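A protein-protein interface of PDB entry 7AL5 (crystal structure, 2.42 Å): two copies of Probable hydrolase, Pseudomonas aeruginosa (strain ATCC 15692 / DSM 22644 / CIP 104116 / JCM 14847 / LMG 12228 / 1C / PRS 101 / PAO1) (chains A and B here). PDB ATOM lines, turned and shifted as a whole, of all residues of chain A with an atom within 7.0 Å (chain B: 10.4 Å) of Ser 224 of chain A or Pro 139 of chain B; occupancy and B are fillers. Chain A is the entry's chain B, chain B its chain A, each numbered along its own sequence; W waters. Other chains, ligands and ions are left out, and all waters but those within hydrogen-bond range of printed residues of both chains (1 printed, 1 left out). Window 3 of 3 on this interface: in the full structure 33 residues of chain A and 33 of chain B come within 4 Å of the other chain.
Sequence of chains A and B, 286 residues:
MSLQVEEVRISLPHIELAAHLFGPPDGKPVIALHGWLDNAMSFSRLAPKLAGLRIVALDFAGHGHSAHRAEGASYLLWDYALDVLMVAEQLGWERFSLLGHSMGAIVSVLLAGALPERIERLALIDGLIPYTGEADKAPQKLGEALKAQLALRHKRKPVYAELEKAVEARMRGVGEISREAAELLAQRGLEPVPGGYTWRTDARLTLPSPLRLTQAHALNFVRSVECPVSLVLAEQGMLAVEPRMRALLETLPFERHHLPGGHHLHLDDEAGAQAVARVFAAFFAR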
ATOM      1  N   VAL A 109     -25.529  -5.968 -10.242  1.00  0.00           N
ATOM      2  CA  VAL A 109     -25.497  -6.960 -11.321  1.00  0.00           C
ATOM      3  C   VAL A 109     -24.064  -7.184 -11.788  1.00  0.00           C
ATOM      4  O   VAL A 109     -23.630  -8.330 -12.006  1.00  0.00           O
ATOM      5  CB  VAL A 109     -26.395  -6.516 -12.493  1.00  0.00           C
ATOM      6  CG1 VAL A 109     -26.261  -7.435 -13.690  1.00  0.00           C
ATOM      7  CG2 VAL A 109     -27.831  -6.419 -12.078  1.00  0.00           C
ATOM      8  N   LEU A 110     -23.305  -6.106 -11.947  1.00  0.00           N
ATOM      9  CA  LEU A 110     -21.912  -6.220 -12.419  1.00  0.00           C
ATOM     10  C   LEU A 110     -21.141  -7.064 -11.409  1.00  0.00           C
ATOM     11  O   LEU A 110     -20.386  -7.887 -11.857  1.00  0.00           O
ATOM     12  CB  LEU A 110     -21.231  -4.858 -12.586  1.00  0.00           C
ATOM     13  CG  LEU A 110     -21.664  -3.973 -13.743  1.00  0.00           C
ATOM     14  CD1 LEU A 110     -20.757  -2.774 -13.847  1.00  0.00           C
ATOM     15  CD2 LEU A 110     -21.721  -4.727 -15.057  1.00  0.00           C
ATOM     16  N   ALA A 112     -22.250  -9.372  -9.087  1.00  0.00           N
ATOM     17  CA  ALA A 112     -22.686 -10.767  -9.134  1.00  0.00           C
ATOM     18  C   ALA A 112     -22.140 -11.459 -10.377  1.00  0.00           C
ATOM     19  O   ALA A 112     -21.594 -12.567 -10.299  1.00  0.00           O
ATOM     20  CB  ALA A 112     -24.224 -10.846  -9.100  1.00  0.00           C
ATOM     21  N   GLY A 113     -22.284 -10.816 -11.540  1.00  0.00           N
ATOM     22  CA  GLY A 113     -21.876 -11.455 -12.777  1.00  0.00           C
ATOM     23  C   GLY A 113     -20.382 -11.693 -12.848  1.00  0.00           C
ATOM     24  O   GLY A 113     -19.918 -12.609 -13.539  1.00  0.00           O
ATOM     25  N   ALA A 114     -19.614 -10.888 -12.136  1.00  0.00           N
ATOM     26  CA  ALA A 114     -18.170 -10.976 -12.199  1.00  0.00           C
ATOM     27  C   ALA A 114     -17.588 -11.833 -11.088  1.00  0.00           C
ATOM     28  O   ALA A 114     -16.509 -12.407 -11.271  1.00  0.00           O
ATOM     29  CB  ALA A 114     -17.573  -9.565 -12.139  1.00  0.00           C
ATOM     30  N   LEU A 115     -18.292 -11.938  -9.955  1.00  0.00           N
ATOM     31  CA  LEU A 115     -17.823 -12.692  -8.794  1.00  0.00           C
ATOM     32  C   LEU A 115     -18.989 -13.501  -8.237  1.00  0.00           C
ATOM     33  O   LEU A 115     -19.445 -13.284  -7.106  1.00  0.00           O
ATOM     34  CB  LEU A 115     -17.243 -11.756  -7.735  1.00  0.00           C
ATOM     35  CG  LEU A 115     -15.984 -11.006  -8.144  1.00  0.00           C
ATOM     36  CD1 LEU A 115     -15.467 -10.084  -7.051  1.00  0.00           C
ATOM     37  CD2 LEU A 115     -14.908 -11.995  -8.521  1.00  0.00           C
ATOM     38  N   PRO A 116     -19.490 -14.461  -9.012  1.00  0.00           N
ATOM     39  CA  PRO A 116     -20.608 -15.285  -8.517  1.00  0.00           C
ATOM     40  C   PRO A 116     -20.333 -15.900  -7.168  1.00  0.00           C
ATOM     41  O   PRO A 116     -21.277 -16.107  -6.405  1.00  0.00           O
ATOM     42  CB  PRO A 116     -20.781 -16.368  -9.591  1.00  0.00           C
ATOM     43  CG  PRO A 116     -20.058 -15.831 -10.803  1.00  0.00           C
ATOM     44  CD  PRO A 116     -19.020 -14.854 -10.351  1.00  0.00           C
ATOM     45  N   HIS A 217     -22.176  -6.646 -23.986  1.00  0.00           N
ATOM     46  CA  HIS A 217     -21.619  -6.672 -22.633  1.00  0.00           C
ATOM     47  C   HIS A 217     -22.736  -6.769 -21.611  1.00  0.00           C
ATOM     48  O   HIS A 217     -22.762  -7.682 -20.784  1.00  0.00           O
ATOM     49  CB  HIS A 217     -20.763  -5.432 -22.352  1.00  0.00           C
ATOM     50  CG  HIS A 217     -19.421  -5.460 -23.004  1.00  0.00           C
ATOM     51  ND1 HIS A 217     -19.098  -4.643 -24.060  1.00  0.00           N
ATOM     52  CD2 HIS A 217     -18.316  -6.191 -22.743  1.00  0.00           C
ATOM     53  CE1 HIS A 217     -17.865  -4.898 -24.450  1.00  0.00           C
ATOM     54  NE2 HIS A 217     -17.353  -5.799 -23.638  1.00  0.00           N
ATOM     55  N   ALA A 218     -23.684  -5.844 -21.676  1.00  0.00           N
ATOM     56  CA  ALA A 218     -24.749  -5.814 -20.693  1.00  0.00           C
ATOM     57  C   ALA A 218     -25.454  -7.160 -20.629  1.00  0.00           C
ATOM     58  O   ALA A 218     -25.601  -7.741 -19.552  1.00  0.00           O
ATOM     59  CB  ALA A 218     -25.720  -4.684 -21.030  1.00  0.00           C
ATOM     60  N   LEU A 219     -25.847  -7.696 -21.785  1.00  0.00           N
ATOM     61  CA  LEU A 219     -26.516  -8.992 -21.822  1.00  0.00           C
ATOM     62  C   LEU A 219     -25.664 -10.076 -21.167  1.00  0.00           C
ATOM     63  O   LEU A 219     -26.165 -10.858 -20.350  1.00  0.00           O
ATOM     64  CB  LEU A 219     -26.848  -9.361 -23.280  1.00  0.00           C
ATOM     65  CG  LEU A 219     -27.963  -8.490 -23.876  1.00  0.00           C
ATOM     66  CD1 LEU A 219     -28.190  -8.862 -25.320  1.00  0.00           C
ATOM     67  CD2 LEU A 219     -29.270  -8.593 -23.120  1.00  0.00           C
ATOM     68  N   ASN A 220     -24.386 -10.095 -21.487  1.00  0.00           N
ATOM     69  CA  ASN A 220     -23.433 -11.063 -20.915  1.00  0.00           C
ATOM     70  C   ASN A 220     -23.340 -10.897 -19.391  1.00  0.00           C
ATOM     71  O   ASN A 220     -23.082 -11.899 -18.765  1.00  0.00           O
ATOM     72  CB  ASN A 220     -22.076 -10.954 -21.587  1.00  0.00           C
ATOM     73  CG  ASN A 220     -21.809 -12.066 -22.568  1.00  0.00           C
ATOM     74  OD1 ASN A 220     -21.328 -13.121 -22.177  1.00  0.00           O
ATOM     75  ND2 ASN A 220     -22.065 -11.825 -23.835  1.00  0.00           N
ATOM     76  N   PHE A 221     -23.584  -9.706 -18.812  1.00  0.00           N
ATOM     77  CA  PHE A 221     -23.448  -9.556 -17.370  1.00  0.00           C
ATOM     78  C   PHE A 221     -24.666 -10.107 -16.654  1.00  0.00           C
ATOM     79  O   PHE A 221     -24.533 -10.843 -15.669  1.00  0.00           O
ATOM     80  CB  PHE A 221     -23.208  -8.080 -16.997  1.00  0.00           C
ATOM     81  CG  PHE A 221     -21.773  -7.753 -16.816  1.00  0.00           C
ATOM     82  CD1 PHE A 221     -21.109  -8.116 -15.647  1.00  0.00           C
ATOM     83  CD2 PHE A 221     -21.052  -7.155 -17.834  1.00  0.00           C
ATOM     84  CE1 PHE A 221     -19.760  -7.860 -15.486  1.00  0.00           C
ATOM     85  CE2 PHE A 221     -19.690  -6.888 -17.681  1.00  0.00           C
ATOM     86  CZ  PHE A 221     -19.042  -7.255 -16.492  1.00  0.00           C
ATOM     87  N   VAL A 222     -25.862  -9.740 -17.107  1.00  0.00           N
ATOM     88  CA  VAL A 222     -27.163 -10.157 -16.510  1.00  0.00           C
ATOM     89  C   VAL A 222     -27.279 -11.667 -16.589  1.00  0.00           C
ATOM     90  O   VAL A 222     -27.664 -12.280 -15.630  1.00  0.00           O
ATOM     91  CB  VAL A 222     -28.397  -9.533 -17.182  1.00  0.00           C
ATOM     92  CG1 VAL A 222     -28.744  -8.190 -16.601  1.00  0.00           C
ATOM     93  CG2 VAL A 222     -28.293  -9.456 -18.682  1.00  0.00           C
ATOM     94  N   ARG A 223     -26.829 -12.235 -17.693  1.00  0.00           N
ATOM     95  CA  ARG A 223     -26.897 -13.680 -17.979  1.00  0.00           C
ATOM     96  C   ARG A 223     -25.803 -14.445 -17.229  1.00  0.00           C
ATOM     97  O   ARG A 223     -25.828 -15.647 -17.322  1.00  0.00           O
ATOM     98  CB  ARG A 223     -26.821 -13.902 -19.490  1.00  0.00           C
ATOM     99  CG  ARG A 223     -28.105 -13.588 -20.241  1.00  0.00           C
ATOM    100  CD  ARG A 223     -27.969 -13.924 -21.706  1.00  0.00           C
ATOM    101  NE  ARG A 223     -28.991 -13.406 -22.604  1.00  0.00           N
ATOM    102  CZ  ARG A 223     -30.299 -13.628 -22.506  1.00  0.00           C
ATOM    103  NH1 ARG A 223     -30.805 -14.337 -21.509  1.00  0.00           N
ATOM    104  NH2 ARG A 223     -31.102 -13.115 -23.413  1.00  0.00           N
ATOM    105  N   SER A 224     -24.845 -13.778 -16.585  1.00  0.00           N
ATOM    106  CA  SER A 224     -23.782 -14.399 -15.768  1.00  0.00           C
ATOM    107  C   SER A 224     -24.148 -14.339 -14.286  1.00  0.00           C
ATOM    108  O   SER A 224     -23.384 -14.836 -13.511  1.00  0.00           O
ATOM    109  CB  SER A 224     -22.461 -13.770 -16.040  1.00  0.00           C
ATOM    110  OG  SER A 224     -22.213 -13.748 -17.419  1.00  0.00           O
ATOM    111  N   VAL A 225     -25.263 -13.727 -13.918  1.00  0.00           N
ATOM    112  CA  VAL A 225     -25.712 -13.706 -12.527  1.00  0.00           C
ATOM    113  C   VAL A 225     -26.196 -15.106 -12.149  1.00  0.00           C
ATOM    114  O   VAL A 225     -27.218 -15.580 -12.650  1.00  0.00           O
ATOM    115  CB  VAL A 225     -26.815 -12.662 -12.324  1.00  0.00           C
ATOM    116  CG1 VAL A 225     -27.398 -12.724 -10.906  1.00  0.00           C
ATOM    117  CG2 VAL A 225     -26.274 -11.264 -12.672  1.00  0.00           C
ATOM    118  N   GLU A 226     -25.469 -15.764 -11.250  1.00  0.00           N
ATOM    119  CA  GLU A 226     -25.749 -17.133 -10.855  1.00  0.00           C
ATOM    120  C   GLU A 226     -26.627 -17.250  -9.607  1.00  0.00           C
ATOM    121  O   GLU A 226     -26.982 -18.357  -9.207  1.00  0.00           O
ATOM    122  CB  GLU A 226     -24.445 -17.865 -10.602  1.00  0.00           C
ATOM    123  CG  GLU A 226     -23.582 -18.122 -11.826  1.00  0.00           C
ATOM    124  CD  GLU A 226     -22.303 -18.885 -11.456  1.00  0.00           C
ATOM    125  OE1 GLU A 226     -22.348 -19.667 -10.480  1.00  0.00           O
ATOM    126  OE2 GLU A 226     -21.248 -18.691 -12.120  1.00  0.00           O
ATOM    127  N   CYS A 227     -26.987 -16.159  -8.980  1.00  0.00           N
ATOM    128  CA  CYS A 227     -27.684 -16.214  -7.711  1.00  0.00           C
ATOM    129  C   CYS A 227     -29.136 -15.829  -7.900  1.00  0.00           C
ATOM    130  O   CYS A 227     -29.515 -15.285  -8.939  1.00  0.00           O
ATOM    131  CB  CYS A 227     -27.015 -15.273  -6.698  1.00  0.00           C
ATOM    132  SG  CYS A 227     -27.081 -13.518  -7.187  1.00  0.00           S
ATOM    133  N   LEU A 252     -35.127 -14.209 -18.544  1.00  0.00           N
ATOM    134  CA  LEU A 252     -34.184 -14.261 -17.425  1.00  0.00           C
ATOM    135  C   LEU A 252     -34.813 -14.884 -16.188  1.00  0.00           C
ATOM    136  O   LEU A 252     -35.979 -14.616 -15.880  1.00  0.00           O
ATOM    137  CB  LEU A 252     -33.660 -12.866 -17.049  1.00  0.00           C
ATOM    138  CG  LEU A 252     -32.708 -12.228 -18.072  1.00  0.00           C
ATOM    139  CD1 LEU A 252     -32.347 -10.785 -17.765  1.00  0.00           C
ATOM    140  CD2 LEU A 252     -31.463 -13.064 -18.192  1.00  0.00           C
ATOM    141  N   PHE A 254     -35.096 -14.246 -13.255  1.00  0.00           N
ATOM    142  CA  PHE A 254     -35.229 -13.341 -12.127  1.00  0.00           C
ATOM    143  C   PHE A 254     -36.696 -13.261 -11.732  1.00  0.00           C
ATOM    144  O   PHE A 254     -37.588 -13.321 -12.588  1.00  0.00           O
ATOM    145  CB  PHE A 254     -34.699 -11.944 -12.469  1.00  0.00           C
ATOM    146  CG  PHE A 254     -33.260 -11.914 -12.977  1.00  0.00           C
ATOM    147  CD1 PHE A 254     -32.382 -12.976 -12.744  1.00  0.00           C
ATOM    148  CD2 PHE A 254     -32.778 -10.795 -13.645  1.00  0.00           C
ATOM    149  CE1 PHE A 254     -31.066 -12.930 -13.203  1.00  0.00           C
ATOM    150  CE2 PHE A 254     -31.470 -10.755 -14.125  1.00  0.00           C
ATOM    151  CZ  PHE A 254     -30.609 -11.817 -13.902  1.00  0.00           C
ATOM    152  N   GLY B 133     -10.679  -7.687 -26.208  1.00  0.00           N
ATOM    153  CA  GLY B 133     -11.400  -8.772 -25.583  1.00  0.00           C
ATOM    154  C   GLY B 133     -12.889  -8.615 -25.796  1.00  0.00           C
ATOM    155  O   GLY B 133     -13.424  -7.504 -25.733  1.00  0.00           O
ATOM    156  N   GLU B 134     -13.566  -9.721 -26.045  1.00  0.00           N
ATOM    157  CA  GLU B 134     -14.939  -9.680 -26.481  1.00  0.00           C
ATOM    158  C   GLU B 134     -15.865  -9.779 -25.291  1.00  0.00           C
ATOM    159  O   GLU B 134     -15.461 -10.102 -24.173  1.00  0.00           O
ATOM    160  CB  GLU B 134     -15.180 -10.784 -27.494  1.00  0.00           C
ATOM    161  CG  GLU B 134     -14.233 -10.630 -28.668  1.00  0.00           C
ATOM    162  CD  GLU B 134     -14.408  -9.277 -29.293  1.00  0.00           C
ATOM    163  OE1 GLU B 134     -15.580  -8.890 -29.494  1.00  0.00           O
ATOM    164  OE2 GLU B 134     -13.399  -8.589 -29.518  1.00  0.00           O
ATOM    165  N   ALA B 135     -17.130  -9.484 -25.552  1.00  0.00           N
ATOM    166  CA  ALA B 135     -18.108  -9.399 -24.476  1.00  0.00           C
ATOM    167  C   ALA B 135     -18.277 -10.719 -23.746  1.00  0.00           C
ATOM    168  O   ALA B 135     -18.612 -10.718 -22.560  1.00  0.00           O
ATOM    169  CB  ALA B 135     -19.457  -8.929 -25.042  1.00  0.00           C
ATOM    170  N   ASP B 136     -18.090 -11.852 -24.433  1.00  0.00           N
ATOM    171  CA  ASP B 136     -18.371 -13.138 -23.796  1.00  0.00           C
ATOM    172  C   ASP B 136     -17.434 -13.390 -22.619  1.00  0.00           C
ATOM    173  O   ASP B 136     -17.795 -14.101 -21.684  1.00  0.00           O
ATOM    174  CB  ASP B 136     -18.300 -14.293 -24.815  1.00  0.00           C
ATOM    175  CG  ASP B 136     -17.060 -14.265 -25.680  1.00  0.00           C
ATOM    176  OD1 ASP B 136     -15.998 -13.812 -25.222  1.00  0.00           O
ATOM    177  OD2 ASP B 136     -17.152 -14.699 -26.847  1.00  0.00           O
ATOM    178  N   LYS B 137     -16.273 -12.775 -22.627  1.00  0.00           N
ATOM    179  CA  LYS B 137     -15.293 -12.933 -21.545  1.00  0.00           C
ATOM    180  C   LYS B 137     -15.308 -11.732 -20.612  1.00  0.00           C
ATOM    181  O   LYS B 137     -14.542 -11.777 -19.696  1.00  0.00           O
ATOM    182  CB  LYS B 137     -13.897 -13.097 -22.132  1.00  0.00           C
ATOM    183  CG  LYS B 137     -13.714 -14.330 -22.984  1.00  0.00           C
ATOM    184  CD  LYS B 137     -13.923 -15.590 -22.212  1.00  0.00           C
ATOM    185  CE  LYS B 137     -13.092 -16.738 -22.729  1.00  0.00           C
ATOM    186  NZ  LYS B 137     -11.702 -16.316 -23.020  1.00  0.00           N
ATOM    187  N   ALA B 138     -16.194 -10.754 -20.775  1.00  0.00           N
ATOM    188  CA  ALA B 138     -16.074  -9.538 -19.973  1.00  0.00           C
ATOM    189  C   ALA B 138     -16.327  -9.784 -18.495  1.00  0.00           C
ATOM    190  O   ALA B 138     -15.486  -9.385 -17.674  1.00  0.00           O
ATOM    191  CB  ALA B 138     -17.004  -8.452 -20.515  1.00  0.00           C
ATOM    192  N   PRO B 139     -17.425 -10.417 -18.084  1.00  0.00           N
ATOM    193  CA  PRO B 139     -17.629 -10.651 -16.637  1.00  0.00           C
ATOM    194  C   PRO B 139     -16.447 -11.348 -16.004  1.00  0.00           C
ATOM    195  O   PRO B 139     -15.973 -10.963 -14.924  1.00  0.00           O
ATOM    196  CB  PRO B 139     -18.894 -11.523 -16.599  1.00  0.00           C
ATOM    197  CG  PRO B 139     -19.565 -11.244 -17.948  1.00  0.00           C
ATOM    198  CD  PRO B 139     -18.435 -11.103 -18.906  1.00  0.00           C
ATOM    199  N   GLN B 140     -15.926 -12.360 -16.694  1.00  0.00           N
ATOM    200  CA  GLN B 140     -14.759 -13.056 -16.182  1.00  0.00           C
ATOM    201  C   GLN B 140     -13.586 -12.097 -16.001  1.00  0.00           C
ATOM    202  O   GLN B 140     -12.876 -12.163 -14.997  1.00  0.00           O
ATOM    203  CB  GLN B 140     -14.393 -14.196 -17.118  1.00  0.00           C
ATOM    204  CG  GLN B 140     -13.206 -14.963 -16.632  1.00  0.00           C
ATOM    205  CD  GLN B 140     -12.869 -16.141 -17.518  1.00  0.00           C
ATOM    206  OE1 GLN B 140     -12.250 -15.978 -18.576  1.00  0.00           O
ATOM    207  NE2 GLN B 140     -13.275 -17.345 -17.087  1.00  0.00           N
ATOM    208  N   LYS B 141     -13.337 -11.239 -16.987  1.00  0.00           N
ATOM    209  CA  LYS B 141     -12.213 -10.270 -17.015  1.00  0.00           C
ATOM    210  C   LYS B 141     -12.341  -9.229 -15.910  1.00  0.00           C
ATOM    211  O   LYS B 141     -11.361  -8.987 -15.254  1.00  0.00           O
ATOM    212  CB  LYS B 141     -12.157  -9.529 -18.344  1.00  0.00           C
ATOM    213  CG  LYS B 141     -11.517 -10.280 -19.484  1.00  0.00           C
ATOM    214  CD  LYS B 141     -10.245 -10.956 -19.130  1.00  0.00           C
ATOM    215  CE  LYS B 141      -9.985 -12.148 -20.012  1.00  0.00           C
ATOM    216  NZ  LYS B 141      -8.563 -12.540 -19.980  1.00  0.00           N
ATOM    217  N   LEU B 142     -13.508  -8.629 -15.741  1.00  0.00           N
ATOM    218  CA  LEU B 142     -13.758  -7.752 -14.611  1.00  0.00           C
ATOM    219  C   LEU B 142     -13.528  -8.504 -13.307  1.00  0.00           C
ATOM    220  O   LEU B 142     -12.844  -8.007 -12.412  1.00  0.00           O
ATOM    221  CB  LEU B 142     -15.170  -7.175 -14.685  1.00  0.00           C
ATOM    222  CG  LEU B 142     -15.615  -6.312 -13.506  1.00  0.00           C
ATOM    223  CD1 LEU B 142     -14.660  -5.174 -13.376  1.00  0.00           C
ATOM    224  CD2 LEU B 142     -17.052  -5.821 -13.643  1.00  0.00           C
ATOM    225  N   GLY B 143     -14.055  -9.722 -13.195  1.00  0.00           N
ATOM    226  CA  GLY B 143     -13.802 -10.511 -11.997  1.00  0.00           C
ATOM    227  C   GLY B 143     -12.318 -10.657 -11.705  1.00  0.00           C
ATOM    228  O   GLY B 143     -11.866 -10.480 -10.569  1.00  0.00           O
ATOM    229  N   GLU B 144     -11.541 -11.002 -12.728  1.00  0.00           N
ATOM    230  CA  GLU B 144     -10.096 -11.045 -12.566  1.00  0.00           C
ATOM    231  C   GLU B 144      -9.568  -9.700 -12.111  1.00  0.00           C
ATOM    232  O   GLU B 144      -8.687  -9.625 -11.244  1.00  0.00           O
ATOM    233  CB  GLU B 144      -9.433 -11.439 -13.878  1.00  0.00           C
ATOM    234  CG  GLU B 144      -9.878 -12.781 -14.433  1.00  0.00           C
ATOM    235  CD  GLU B 144      -9.113 -13.122 -15.693  1.00  0.00           C
ATOM    236  OE1 GLU B 144      -9.350 -14.199 -16.273  1.00  0.00           O
ATOM    237  OE2 GLU B 144      -8.274 -12.288 -16.109  1.00  0.00           O
ATOM    238  N   ALA B 145     -10.050  -8.612 -12.681  1.00  0.00           N
ATOM    239  CA  ALA B 145      -9.560  -7.258 -12.353  1.00  0.00           C
ATOM    240  C   ALA B 145      -9.843  -6.918 -10.887  1.00  0.00           C
ATOM    241  O   ALA B 145      -8.991  -6.322 -10.291  1.00  0.00           O
ATOM    242  CB  ALA B 145     -10.123  -6.234 -13.302  1.00  0.00           C
ATOM    243  N   LEU B 146     -11.011  -7.267 -10.361  1.00  0.00           N
ATOM    244  CA  LEU B 146     -11.427  -7.009  -8.966  1.00  0.00           C
ATOM    245  C   LEU B 146     -10.533  -7.794  -8.001  1.00  0.00           C
ATOM    246  O   LEU B 146     -10.124  -7.243  -7.001  1.00  0.00           O
ATOM    247  CB  LEU B 146     -12.891  -7.416  -8.811  1.00  0.00           C
ATOM    248  CG  LEU B 146     -13.976  -6.381  -9.086  1.00  0.00           C
ATOM    249  CD1 LEU B 146     -13.421  -5.035  -9.476  1.00  0.00           C
ATOM    250  CD2 LEU B 146     -14.930  -6.880 -10.148  1.00  0.00           C
ATOM    251  N   LYS B 147     -10.256  -9.051  -8.322  1.00  0.00           N
ATOM    252  CA  LYS B 147      -9.397  -9.953  -7.529  1.00  0.00           C
ATOM    253  C   LYS B 147      -7.974  -9.392  -7.523  1.00  0.00           C
ATOM    254  O   LYS B 147      -7.371  -9.368  -6.482  1.00  0.00           O
ATOM    255  CB  LYS B 147      -9.462 -11.380  -8.081  1.00  0.00           C
ATOM    256  CG  LYS B 147     -10.457 -12.290  -7.392  1.00  0.00           C
ATOM    257  CD  LYS B 147     -11.441 -12.944  -8.314  1.00  0.00           C
ATOM    258  CE  LYS B 147     -11.181 -14.414  -8.560  1.00  0.00           C
ATOM    259  NZ  LYS B 147     -12.414 -15.124  -8.971  1.00  0.00           N
ATOM    260  N   PRO B 208      -4.848  -5.993 -14.530  1.00  0.00           N
ATOM    261  CA  PRO B 208      -5.580  -6.213 -15.783  1.00  0.00           C
ATOM    262  C   PRO B 208      -6.601  -5.100 -15.960  1.00  0.00           C
ATOM    263  O   PRO B 208      -7.069  -4.489 -14.993  1.00  0.00           O
ATOM    264  CB  PRO B 208      -6.322  -7.531 -15.554  1.00  0.00           C
ATOM    265  CG  PRO B 208      -5.704  -8.132 -14.299  1.00  0.00           C
ATOM    266  CD  PRO B 208      -5.253  -6.949 -13.484  1.00  0.00           C
ATOM    267  N   SER B 209      -7.003  -4.877 -17.199  1.00  0.00           N
ATOM    268  CA  SER B 209      -8.081  -3.928 -17.454  1.00  0.00           C
ATOM    269  C   SER B 209      -9.387  -4.459 -16.878  1.00  0.00           C
ATOM    270  O   SER B 209      -9.686  -5.656 -16.984  1.00  0.00           O
ATOM    271  CB  SER B 209      -8.245  -3.688 -18.952  1.00  0.00           C
ATOM    272  OG  SER B 209      -9.110  -2.594 -19.198  1.00  0.00           O
ATOM    273  N   PRO B 210     -10.178  -3.611 -16.234  1.00  0.00           N
ATOM    274  CA  PRO B 210     -11.532  -4.062 -15.864  1.00  0.00           C
ATOM    275  C   PRO B 210     -12.401  -4.265 -17.077  1.00  0.00           C
ATOM    276  O   PRO B 210     -13.315  -5.090 -17.017  1.00  0.00           O
ATOM    277  CB  PRO B 210     -12.066  -2.947 -14.953  1.00  0.00           C
ATOM    278  CG  PRO B 210     -11.256  -1.707 -15.375  1.00  0.00           C
ATOM    279  CD  PRO B 210      -9.925  -2.183 -15.927  1.00  0.00           C
ATOM    280  N   LEU B 211     -12.138  -3.561 -18.191  1.00  0.00           N
ATOM    281  CA  LEU B 211     -13.012  -3.646 -19.370  1.00  0.00           C
ATOM    282  C   LEU B 211     -12.172  -3.392 -20.618  1.00  0.00           C
ATOM    283  O   LEU B 211     -11.842  -2.241 -20.917  1.00  0.00           O
ATOM    284  CB  LEU B 211     -14.166  -2.657 -19.286  1.00  0.00           C
ATOM    285  CG  LEU B 211     -15.033  -2.584 -20.552  1.00  0.00           C
ATOM    286  CD1 LEU B 211     -16.001  -3.760 -20.677  1.00  0.00           C
ATOM    287  CD2 LEU B 211     -15.809  -1.258 -20.630  1.00  0.00           C
ATOM    288  N   ARG B 212     -11.869  -4.459 -21.355  1.00  0.00           N
ATOM    289  CA  ARG B 212     -11.080  -4.366 -22.569  1.00  0.00           C
ATOM    290  C   ARG B 212     -11.910  -3.831 -23.723  1.00  0.00           C
ATOM    291  O   ARG B 212     -13.125  -4.058 -23.801  1.00  0.00           O
ATOM    292  CB  ARG B 212     -10.515  -5.738 -22.947  1.00  0.00           C
ATOM    293  CG  ARG B 212      -9.091  -5.932 -22.439  1.00  0.00           C
ATOM    294  CD  ARG B 212      -8.538  -7.301 -22.719  1.00  0.00           C
ATOM    295  NE  ARG B 212      -7.103  -7.250 -22.987  1.00  0.00           N
ATOM    296  CZ  ARG B 212      -6.238  -8.179 -22.580  1.00  0.00           C
ATOM    297  NH1 ARG B 212      -6.668  -9.230 -21.883  1.00  0.00           N
ATOM    298  NH2 ARG B 212      -4.943  -8.065 -22.868  1.00  0.00           N
HETATM  299  O   HOH W   1     -14.636  -6.207 -23.694  1.00  0.00           O
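Hydrophobic or aromatic side chains of chain A that line the printed part of chain B: Ala 114, Leu 115, His 217 and Phe 221. Of the 20 printed residues of chain B, 8 touch a printed residue of chain A. Hydrophobic or aromatic side chains of chain B within 4 Å of the printed part of chain A: Ala 135, Ala 138, Pro 139, Leu 142 and Leu 211. Among the printed residues, 14 pairs touch across the chains. Among the printed residues, no Asp or Glu carboxylate lies within 4 Å of a Lys or Arg side-chain nitrogen of the other chain.
Among the printed residues, pairs that only touch across the chains: Asn 220 of chain A with Asp 136 of chain B (3.4 Å), Ala 114 of chain A with Gly 143 of chain B (3.4 Å), Gly 113 of chain A with Pro 139 of chain B (3.4 Å), His 217 of chain A with Ala 138 of chain B (3.4 Å), Asn 220 of chain A with Ala 135 of chain B (3.5 Å), Ala 114 of chain A with Pro 139 of chain B (3.5 Å), Leu 115 of chain A with Lys 147 of chain B (3.6 Å), His 217 of chain A with Ala 135 of chain B (3.7 Å), Asn 220 of chain A with Pro 139 of chain B (3.7 Å), Phe 221 of chain A with Pro 139 of chain B (3.7 Å), Ser 224 of chain A with Pro 139 of chain B (3.7 Å), Phe 221 of chain A with Leu 142 of chain B (3.8 Å), His 217 of chain A with Leu 211 of chain B (3.8 Å) and Leu 115 of chain A with Gly 143 of chain B (3.9 Å).
O of Leu 211 of chain B lies within hydrogen-bond range of OG of Ser 209 of chain B, at 3.2 Å. The side-chain hydroxyl (OG) of Ser 224 of chain A lies within hydrogen-bond range of the backbone carbonyl oxygen (O) of Asn 220 of chain A, 2.4 Å away.
Ser 224 of chain A touches just one residue of chain B: Pro 139 (3.7 Å). Pro 139 of chain B touches just these residues of chain A: Gly 113, Ala 114, Asn 220, Phe 221 and Ser 224. Printed residues of chain B within 4 Å of Gly 113 of chain A: Pro 139 (3.4 Å). Of chain B, only Pro 139 and Gly 143 come within 4 Å of Ala 114 of chain A. Of chain B, only Ala 135, Asp 136 and Pro 139 come within 4 Å of Asn 220 of chain A. Of chain B, only Pro 139 (3.7 Å) and Leu 142 (3.8 Å) come within 4 Å of Phe 221 of chain A. No residue of chain B comes within 4 Å of Val 225 of chain A. Printed residues of chain B within 4 Å of His 217 of chain A: Ala 135, Ala 138 and Leu 211. Printed residues of chain A within 4 Å of Leu 211 of chain B: His 217 (3.8 Å). Ala 145 of chain B touches none of the printed residues of chain A. Phe 254 of chain A touches none of the printed residues of chain B. The nearest residue of chain B that does not touch Ser 224 of chain A is Asp 136 of chain B (6.2 Å). The nearest printed residue of chain A that does not touch Pro 139 of chain B is His 217 of chain A (5.6 Å).
No position is printed for both chains. Of the 14 pairs that touch across the chains among the printed residues, none has its exchanged pair printed and touching as well.
Water W1 lies within hydrogen-bond range of O of Arg 212 of chain B, O of Gly 133 of chain B and NE2 of His 217 of chain A.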
